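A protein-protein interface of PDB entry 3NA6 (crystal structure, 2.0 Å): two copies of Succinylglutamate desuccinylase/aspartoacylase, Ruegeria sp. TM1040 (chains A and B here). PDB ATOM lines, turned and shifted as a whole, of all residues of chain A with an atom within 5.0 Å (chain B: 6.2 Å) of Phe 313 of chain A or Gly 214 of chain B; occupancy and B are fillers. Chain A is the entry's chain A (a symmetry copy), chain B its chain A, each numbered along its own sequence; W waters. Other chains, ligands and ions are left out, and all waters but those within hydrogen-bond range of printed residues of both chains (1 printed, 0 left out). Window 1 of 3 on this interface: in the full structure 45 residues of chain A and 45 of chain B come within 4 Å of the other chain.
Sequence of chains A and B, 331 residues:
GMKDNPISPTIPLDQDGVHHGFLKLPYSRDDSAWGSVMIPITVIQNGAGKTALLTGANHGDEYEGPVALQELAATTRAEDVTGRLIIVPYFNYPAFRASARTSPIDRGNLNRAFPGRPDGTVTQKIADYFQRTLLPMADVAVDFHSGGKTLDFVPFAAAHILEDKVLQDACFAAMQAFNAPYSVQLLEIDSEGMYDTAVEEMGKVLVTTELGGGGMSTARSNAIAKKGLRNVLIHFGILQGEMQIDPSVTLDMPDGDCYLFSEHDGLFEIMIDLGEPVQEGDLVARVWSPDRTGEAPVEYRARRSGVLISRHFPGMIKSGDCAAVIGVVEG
The backbone NH (N) of Gly 315 of chain A sits at hydrogen-bond distance from the backbone carbonyl oxygen (O) of Gly 215 of chain B.
O of Ser 217 of chain B is in hydrogen-bond range of NH1 of Arg 311 of chain A (2.9 Å).
The backbone carbonyl oxygen of Gly 148 of chain B sits at hydrogen-bond distance from the backbone NH of Gly 215 of chain B (3.3 Å).
NE2 of His 312 of chain A sits close to O of Pro 314 of chain A, 3.2 Å away.
O of Thr 150 of chain A sits at hydrogen-bond distance from N of Phe 313 of chain A, 2.9 Å away.
The backbone carbonyl oxygen of Leu 151 of chain A is in hydrogen-bond range of the backbone NH of Gly 214 of chain A, 3.1 Å away.
The backbone carbonyl oxygen (O) of Thr 150 of chain B lies within hydrogen-bond range of the backbone NH (N) of Phe 313 of chain B (2.9 Å).
The backbone NH (N) of Gly 214 of chain B sits at hydrogen-bond distance from the backbone carbonyl oxygen (O) of Gly 148 of chain B, 2.7 Å away.
Among the printed residues, pairs that only touch across the chains: Gly 214 of chain A with Phe 313 of chain B, Arg 311 of chain A with Met 216 of chain B, Phe 313 of chain A with Gly 214 of chain B, Phe 313 of chain A with Met 216 of chain B, Phe 313 of chain A with Phe 313 of chain B and Pro 314 of chain A with Gly 215 of chain B.
Of the printed residues of chain B, Gly 214 of chain A touches Phe 313 (3.5 Å).
Printed residues of chain B within 4 Å of Phe 313 of chain A: Gly 214, Met 216 and Phe 313.
Lys 149 of chain B touches none of the printed residues of chain A.
Of the printed residues of chain A, Gly 215 of chain B touches Pro 314 (3.7 Å) and Gly 315 (3.1 Å).
The nearest printed residue of chain A that does not touch Gly 214 of chain B is Gly 214 of chain A (5.4 Å).
Printed residues of chain B that touch a printed residue of chain A: Gly 214, Gly 215, Met 216, Ser 217 and Phe 313.
Among the printed residues, no Asp or Glu carboxylate lies within 4 Å of a Lys or Arg side-chain nitrogen of the other chain.
Gly 214 of chain A touches Phe 313 of chain B, and with the chains exchanged Phe 313 of chain A touches Gly 214 of chain B.
Phe 313 of chain A touches its own counterpart, Phe 313 of chain B.
Positions printed for both chains: 149, 150, 151, 152, 213, 214 and 313.
Water W1 lies within hydrogen-bond range of the guanidinium group (NH2) of Arg 311 of chain A (2.8 Å), the backbone NH (N) of Ser 217 of chain B (2.9 Å) and the backbone carbonyl oxygen (O) of Phe 313 of chain A (2.9 Å).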
ATOM      1  N   LYS A 149     -24.679  15.121   8.262  1.00  0.00           N
ATOM      2  CA  LYS A 149     -23.992  14.004   7.601  1.00  0.00           C
ATOM      3  C   LYS A 149     -24.785  12.688   7.589  1.00  0.00           C
ATOM      4  O   LYS A 149     -24.573  11.846   6.746  1.00  0.00           O
ATOM      5  CB  LYS A 149     -22.622  13.760   8.254  1.00  0.00           C
ATOM      6  CG  LYS A 149     -21.541  14.741   7.816  1.00  0.00           C
ATOM      7  CD  LYS A 149     -20.241  14.534   8.650  1.00  0.00           C
ATOM      8  CE  LYS A 149     -19.103  15.369   8.077  1.00  0.00           C
ATOM      9  NZ  LYS A 149     -17.910  15.307   8.925  1.00  0.00           N
ATOM     10  N   THR A 150     -25.700  12.524   8.528  1.00  0.00           N
ATOM     11  CA  THR A 150     -26.352  11.249   8.718  1.00  0.00           C
ATOM     12  C   THR A 150     -27.797  11.200   8.219  1.00  0.00           C
ATOM     13  O   THR A 150     -28.392  10.121   8.212  1.00  0.00           O
ATOM     14  CB  THR A 150     -26.308  10.826  10.204  1.00  0.00           C
ATOM     15  OG1 THR A 150     -27.223  11.634  10.957  1.00  0.00           O
ATOM     16  CG2 THR A 150     -24.869  10.990  10.750  1.00  0.00           C
ATOM     17  N   LEU A 151     -28.342  12.326   7.741  1.00  0.00           N
ATOM     18  CA  LEU A 151     -29.765  12.391   7.372  1.00  0.00           C
ATOM     19  C   LEU A 151     -29.982  13.272   6.143  1.00  0.00           C
ATOM     20  O   LEU A 151     -29.232  14.231   5.887  1.00  0.00           O
ATOM     21  CB  LEU A 151     -30.598  12.983   8.516  1.00  0.00           C
ATOM     22  CG  LEU A 151     -30.991  12.181   9.745  1.00  0.00           C
ATOM     23  CD1 LEU A 151     -31.805  13.111  10.641  1.00  0.00           C
ATOM     24  CD2 LEU A 151     -31.794  10.888   9.412  1.00  0.00           C
ATOM     25  N   ASP A 152     -31.048  12.979   5.411  1.00  0.00           N
ATOM     26  CA  ASP A 152     -31.447  13.824   4.265  1.00  0.00           C
ATOM     27  C   ASP A 152     -32.946  13.970   4.298  1.00  0.00           C
ATOM     28  O   ASP A 152     -33.635  13.048   4.671  1.00  0.00           O
ATOM     29  CB  ASP A 152     -30.957  13.191   2.981  1.00  0.00           C
ATOM     30  CG  ASP A 152     -30.868  14.170   1.816  1.00  0.00           C
ATOM     31  OD1 ASP A 152     -31.216  15.358   1.965  1.00  0.00           O
ATOM     32  OD2 ASP A 152     -30.486  13.701   0.718  1.00  0.00           O
ATOM     33  N   GLY A 213     -29.448  17.810   3.276  1.00  0.00           N
ATOM     34  CA  GLY A 213     -28.632  17.040   4.212  1.00  0.00           C
ATOM     35  C   GLY A 213     -27.463  16.345   3.542  1.00  0.00           C
ATOM     36  O   GLY A 213     -27.062  16.716   2.445  1.00  0.00           O
ATOM     37  N   GLY A 214     -26.914  15.348   4.239  1.00  0.00           N
ATOM     38  CA  GLY A 214     -25.759  14.572   3.801  1.00  0.00           C
ATOM     39  C   GLY A 214     -24.454  15.301   4.014  1.00  0.00           C
ATOM     40  O   GLY A 214     -23.408  14.879   3.502  1.00  0.00           O
ATOM     41  N   ARG A 311     -34.530  10.304   5.191  1.00  0.00           N
ATOM     42  CA  ARG A 311     -33.818   9.016   5.136  1.00  0.00           C
ATOM     43  C   ARG A 311     -32.482   9.051   5.843  1.00  0.00           C
ATOM     44  O   ARG A 311     -31.836  10.093   5.890  1.00  0.00           O
ATOM     45  CB  ARG A 311     -33.600   8.559   3.695  1.00  0.00           C
ATOM     46  CG  ARG A 311     -32.930   9.573   2.755  1.00  0.00           C
ATOM     47  CD  ARG A 311     -32.261   8.883   1.536  1.00  0.00           C
ATOM     48  NE  ARG A 311     -31.142   8.024   1.970  1.00  0.00           N
ATOM     49  CZ  ARG A 311     -30.345   7.327   1.153  1.00  0.00           C
ATOM     50  NH1 ARG A 311     -30.524   7.360  -0.151  1.00  0.00           N
ATOM     51  NH2 ARG A 311     -29.363   6.577   1.655  1.00  0.00           N
ATOM     52  N   HIS A 312     -32.078   7.897   6.373  1.00  0.00           N
ATOM     53  CA  HIS A 312     -30.705   7.697   6.809  1.00  0.00           C
ATOM     54  C   HIS A 312     -29.843   7.935   5.587  1.00  0.00           C
ATOM     55  O   HIS A 312     -30.140   7.380   4.527  1.00  0.00           O
ATOM     56  CB  HIS A 312     -30.523   6.252   7.292  1.00  0.00           C
ATOM     57  CG  HIS A 312     -29.118   5.897   7.662  1.00  0.00           C
ATOM     58  ND1 HIS A 312     -28.562   6.217   8.887  1.00  0.00           N
ATOM     59  CD2 HIS A 312     -28.173   5.197   6.988  1.00  0.00           C
ATOM     60  CE1 HIS A 312     -27.321   5.762   8.929  1.00  0.00           C
ATOM     61  NE2 HIS A 312     -27.062   5.131   7.795  1.00  0.00           N
ATOM     62  N   PHE A 313     -28.764   8.706   5.734  1.00  0.00           N
ATOM     63  CA  PHE A 313     -27.902   9.020   4.591  1.00  0.00           C
ATOM     64  C   PHE A 313     -26.745   8.035   4.275  1.00  0.00           C
ATOM     65  O   PHE A 313     -26.678   7.524   3.164  1.00  0.00           O
ATOM     66  CB  PHE A 313     -27.422  10.462   4.727  1.00  0.00           C
ATOM     67  CG  PHE A 313     -26.660  10.969   3.547  1.00  0.00           C
ATOM     68  CD1 PHE A 313     -27.329  11.532   2.488  1.00  0.00           C
ATOM     69  CD2 PHE A 313     -25.279  10.939   3.528  1.00  0.00           C
ATOM     70  CE1 PHE A 313     -26.652  12.017   1.408  1.00  0.00           C
ATOM     71  CE2 PHE A 313     -24.593  11.437   2.449  1.00  0.00           C
ATOM     72  CZ  PHE A 313     -25.301  11.986   1.388  1.00  0.00           C
ATOM     73  N   PRO A 314     -25.860   7.724   5.257  1.00  0.00           N
ATOM     74  CA  PRO A 314     -24.675   6.966   4.937  1.00  0.00           C
ATOM     75  C   PRO A 314     -24.940   5.534   4.487  1.00  0.00           C
ATOM     76  O   PRO A 314     -25.958   4.952   4.819  1.00  0.00           O
ATOM     77  CB  PRO A 314     -23.852   6.982   6.266  1.00  0.00           C
ATOM     78  CG  PRO A 314     -24.384   8.119   7.035  1.00  0.00           C
ATOM     79  CD  PRO A 314     -25.846   8.201   6.651  1.00  0.00           C
ATOM     80  N   GLY A 315     -24.003   4.997   3.714  1.00  0.00           N
ATOM     81  CA  GLY A 315     -24.054   3.642   3.229  1.00  0.00           C
ATOM     82  C   GLY A 315     -24.189   2.606   4.311  1.00  0.00           C
ATOM     83  O   GLY A 315     -24.781   1.563   4.091  1.00  0.00           O
ATOM     84  N   ASP B  61     -15.852   3.329   1.033  1.00  0.00           N
ATOM     85  CA  ASP B  61     -16.947   4.316   1.161  1.00  0.00           C
ATOM     86  C   ASP B  61     -17.751   4.511  -0.141  1.00  0.00           C
ATOM     87  O   ASP B  61     -18.319   5.596  -0.407  1.00  0.00           O
ATOM     88  CB  ASP B  61     -16.407   5.645   1.734  1.00  0.00           C
ATOM     89  CG  ASP B  61     -15.336   6.326   0.844  1.00  0.00           C
ATOM     90  OD1 ASP B  61     -14.787   5.690  -0.083  1.00  0.00           O
ATOM     91  OD2 ASP B  61     -15.056   7.535   1.065  1.00  0.00           O
ATOM     92  N   GLY B 147     -17.939   7.901  -6.213  1.00  0.00           N
ATOM     93  CA  GLY B 147     -17.071   8.981  -5.786  1.00  0.00           C
ATOM     94  C   GLY B 147     -16.456   8.857  -4.406  1.00  0.00           C
ATOM     95  O   GLY B 147     -15.350   9.333  -4.175  1.00  0.00           O
ATOM     96  N   GLY B 148     -17.160   8.213  -3.491  1.00  0.00           N
ATOM     97  CA  GLY B 148     -16.740   8.172  -2.102  1.00  0.00           C
ATOM     98  C   GLY B 148     -17.257   9.401  -1.365  1.00  0.00           C
ATOM     99  O   GLY B 148     -17.964  10.224  -1.949  1.00  0.00           O
ATOM    100  N   LYS B 149     -16.844   9.557  -0.104  1.00  0.00           N
ATOM    101  CA  LYS B 149     -17.344  10.636   0.759  1.00  0.00           C
ATOM    102  C   LYS B 149     -17.041  12.051   0.244  1.00  0.00           C
ATOM    103  O   LYS B 149     -17.728  12.990   0.579  1.00  0.00           O
ATOM    104  CB  LYS B 149     -16.778  10.485   2.180  1.00  0.00           C
ATOM    105  CG  LYS B 149     -17.484   9.427   3.020  1.00  0.00           C
ATOM    106  CD  LYS B 149     -16.742   9.218   4.374  1.00  0.00           C
ATOM    107  CE  LYS B 149     -17.557   8.318   5.294  1.00  0.00           C
ATOM    108  NZ  LYS B 149     -16.821   7.985   6.515  1.00  0.00           N
ATOM    109  N   THR B 150     -16.012  12.193  -0.572  1.00  0.00           N
ATOM    110  CA  THR B 150     -15.532  13.502  -0.947  1.00  0.00           C
ATOM    111  C   THR B 150     -15.885  13.919  -2.374  1.00  0.00           C
ATOM    112  O   THR B 150     -15.640  15.069  -2.742  1.00  0.00           O
ATOM    113  CB  THR B 150     -14.003  13.605  -0.745  1.00  0.00           C
ATOM    114  OG1 THR B 150     -13.337  12.847  -1.766  1.00  0.00           O
ATOM    115  CG2 THR B 150     -13.625  13.071   0.657  1.00  0.00           C
ATOM    116  N   LEU B 151     -16.515  13.032  -3.156  1.00  0.00           N
ATOM    117  CA  LEU B 151     -16.765  13.308  -4.581  1.00  0.00           C
ATOM    118  C   LEU B 151     -18.112  12.746  -5.029  1.00  0.00           C
ATOM    119  O   LEU B 151     -18.607  11.735  -4.500  1.00  0.00           O
ATOM    120  CB  LEU B 151     -15.682  12.665  -5.457  1.00  0.00           C
ATOM    121  CG  LEU B 151     -14.295  13.265  -5.622  1.00  0.00           C
ATOM    122  CD1 LEU B 151     -13.521  12.343  -6.560  1.00  0.00           C
ATOM    123  CD2 LEU B 151     -14.312  14.725  -6.166  1.00  0.00           C
ATOM    124  N   ASP B 152     -18.680  13.373  -6.049  1.00  0.00           N
ATOM    125  CA  ASP B 152     -19.926  12.864  -6.666  1.00  0.00           C
ATOM    126  C   ASP B 152     -19.790  12.995  -8.160  1.00  0.00           C
ATOM    127  O   ASP B 152     -19.192  13.936  -8.632  1.00  0.00           O
ATOM    128  CB  ASP B 152     -21.107  13.637  -6.122  1.00  0.00           C
ATOM    129  CG  ASP B 152     -22.437  12.911  -6.287  1.00  0.00           C
ATOM    130  OD1 ASP B 152     -22.481  11.803  -6.858  1.00  0.00           O
ATOM    131  OD2 ASP B 152     -23.456  13.510  -5.874  1.00  0.00           O
ATOM    132  N   GLY B 212     -22.012   7.399  -8.622  1.00  0.00           N
ATOM    133  CA  GLY B 212     -22.563   8.474  -7.805  1.00  0.00           C
ATOM    134  C   GLY B 212     -21.481   8.857  -6.830  1.00  0.00           C
ATOM    135  O   GLY B 212     -20.334   9.114  -7.228  1.00  0.00           O
ATOM    136  N   GLY B 213     -21.809   8.854  -5.553  1.00  0.00           N
ATOM    137  CA  GLY B 213     -20.821   9.255  -4.555  1.00  0.00           C
ATOM    138  C   GLY B 213     -21.449   9.840  -3.306  1.00  0.00           C
ATOM    139  O   GLY B 213     -22.626   9.627  -3.041  1.00  0.00           O
ATOM    140  N   GLY B 214     -20.630  10.557  -2.535  1.00  0.00           N
ATOM    141  CA  GLY B 214     -21.014  11.177  -1.271  1.00  0.00           C
ATOM    142  C   GLY B 214     -21.056  10.189  -0.128  1.00  0.00           C
ATOM    143  O   GLY B 214     -21.569  10.504   0.954  1.00  0.00           O
ATOM    144  N   GLY B 215     -20.523   8.978  -0.320  1.00  0.00           N
ATOM    145  CA  GLY B 215     -20.591   8.001   0.765  1.00  0.00           C
ATOM    146  C   GLY B 215     -21.992   7.444   1.021  1.00  0.00           C
ATOM    147  O   GLY B 215     -22.301   7.020   2.127  1.00  0.00           O
ATOM    148  N   MET B 216     -22.811   7.388  -0.021  1.00  0.00           N
ATOM    149  CA  MET B 216     -24.205   6.980   0.088  1.00  0.00           C
ATOM    150  C   MET B 216     -24.620   6.433  -1.247  1.00  0.00           C
ATOM    151  O   MET B 216     -23.913   6.576  -2.234  1.00  0.00           O
ATOM    152  CB  MET B 216     -25.099   8.180   0.419  1.00  0.00           C
ATOM    153  CG  MET B 216     -25.069   9.274  -0.618  1.00  0.00           C
ATOM    154  SD  MET B 216     -26.456   9.130  -1.976  1.00  0.00           S
ATOM    155  CE  MET B 216     -27.993   9.671  -0.930  1.00  0.00           C
ATOM    156  N   SER B 217     -25.792   5.829  -1.274  1.00  0.00           N
ATOM    157  CA  SER B 217     -26.430   5.502  -2.519  1.00  0.00           C
ATOM    158  C   SER B 217     -27.947   5.652  -2.432  1.00  0.00           C
ATOM    159  O   SER B 217     -28.518   5.595  -1.370  1.00  0.00           O
ATOM    160  CB  SER B 217     -26.046   4.077  -2.948  1.00  0.00           C
ATOM    161  OG  SER B 217     -26.624   3.116  -2.088  1.00  0.00           O
ATOM    162  N   PHE B 313     -17.769  16.994  -2.946  1.00  0.00           N
ATOM    163  CA  PHE B 313     -19.020  16.759  -2.221  1.00  0.00           C
ATOM    164  C   PHE B 313     -19.247  17.555  -0.907  1.00  0.00           C
ATOM    165  O   PHE B 313     -20.245  18.255  -0.795  1.00  0.00           O
ATOM    166  CB  PHE B 313     -19.199  15.255  -2.032  1.00  0.00           C
ATOM    167  CG  PHE B 313     -20.513  14.862  -1.447  1.00  0.00           C
ATOM    168  CD1 PHE B 313     -21.596  14.656  -2.265  1.00  0.00           C
ATOM    169  CD2 PHE B 313     -20.647  14.637  -0.089  1.00  0.00           C
ATOM    170  CE1 PHE B 313     -22.802  14.279  -1.752  1.00  0.00           C
ATOM    171  CE2 PHE B 313     -21.856  14.246   0.429  1.00  0.00           C
ATOM    172  CZ  PHE B 313     -22.934  14.061  -0.426  1.00  0.00           C
HETATM  173  O   HOH W   1     -26.877   5.219   1.352  1.00  0.00           O
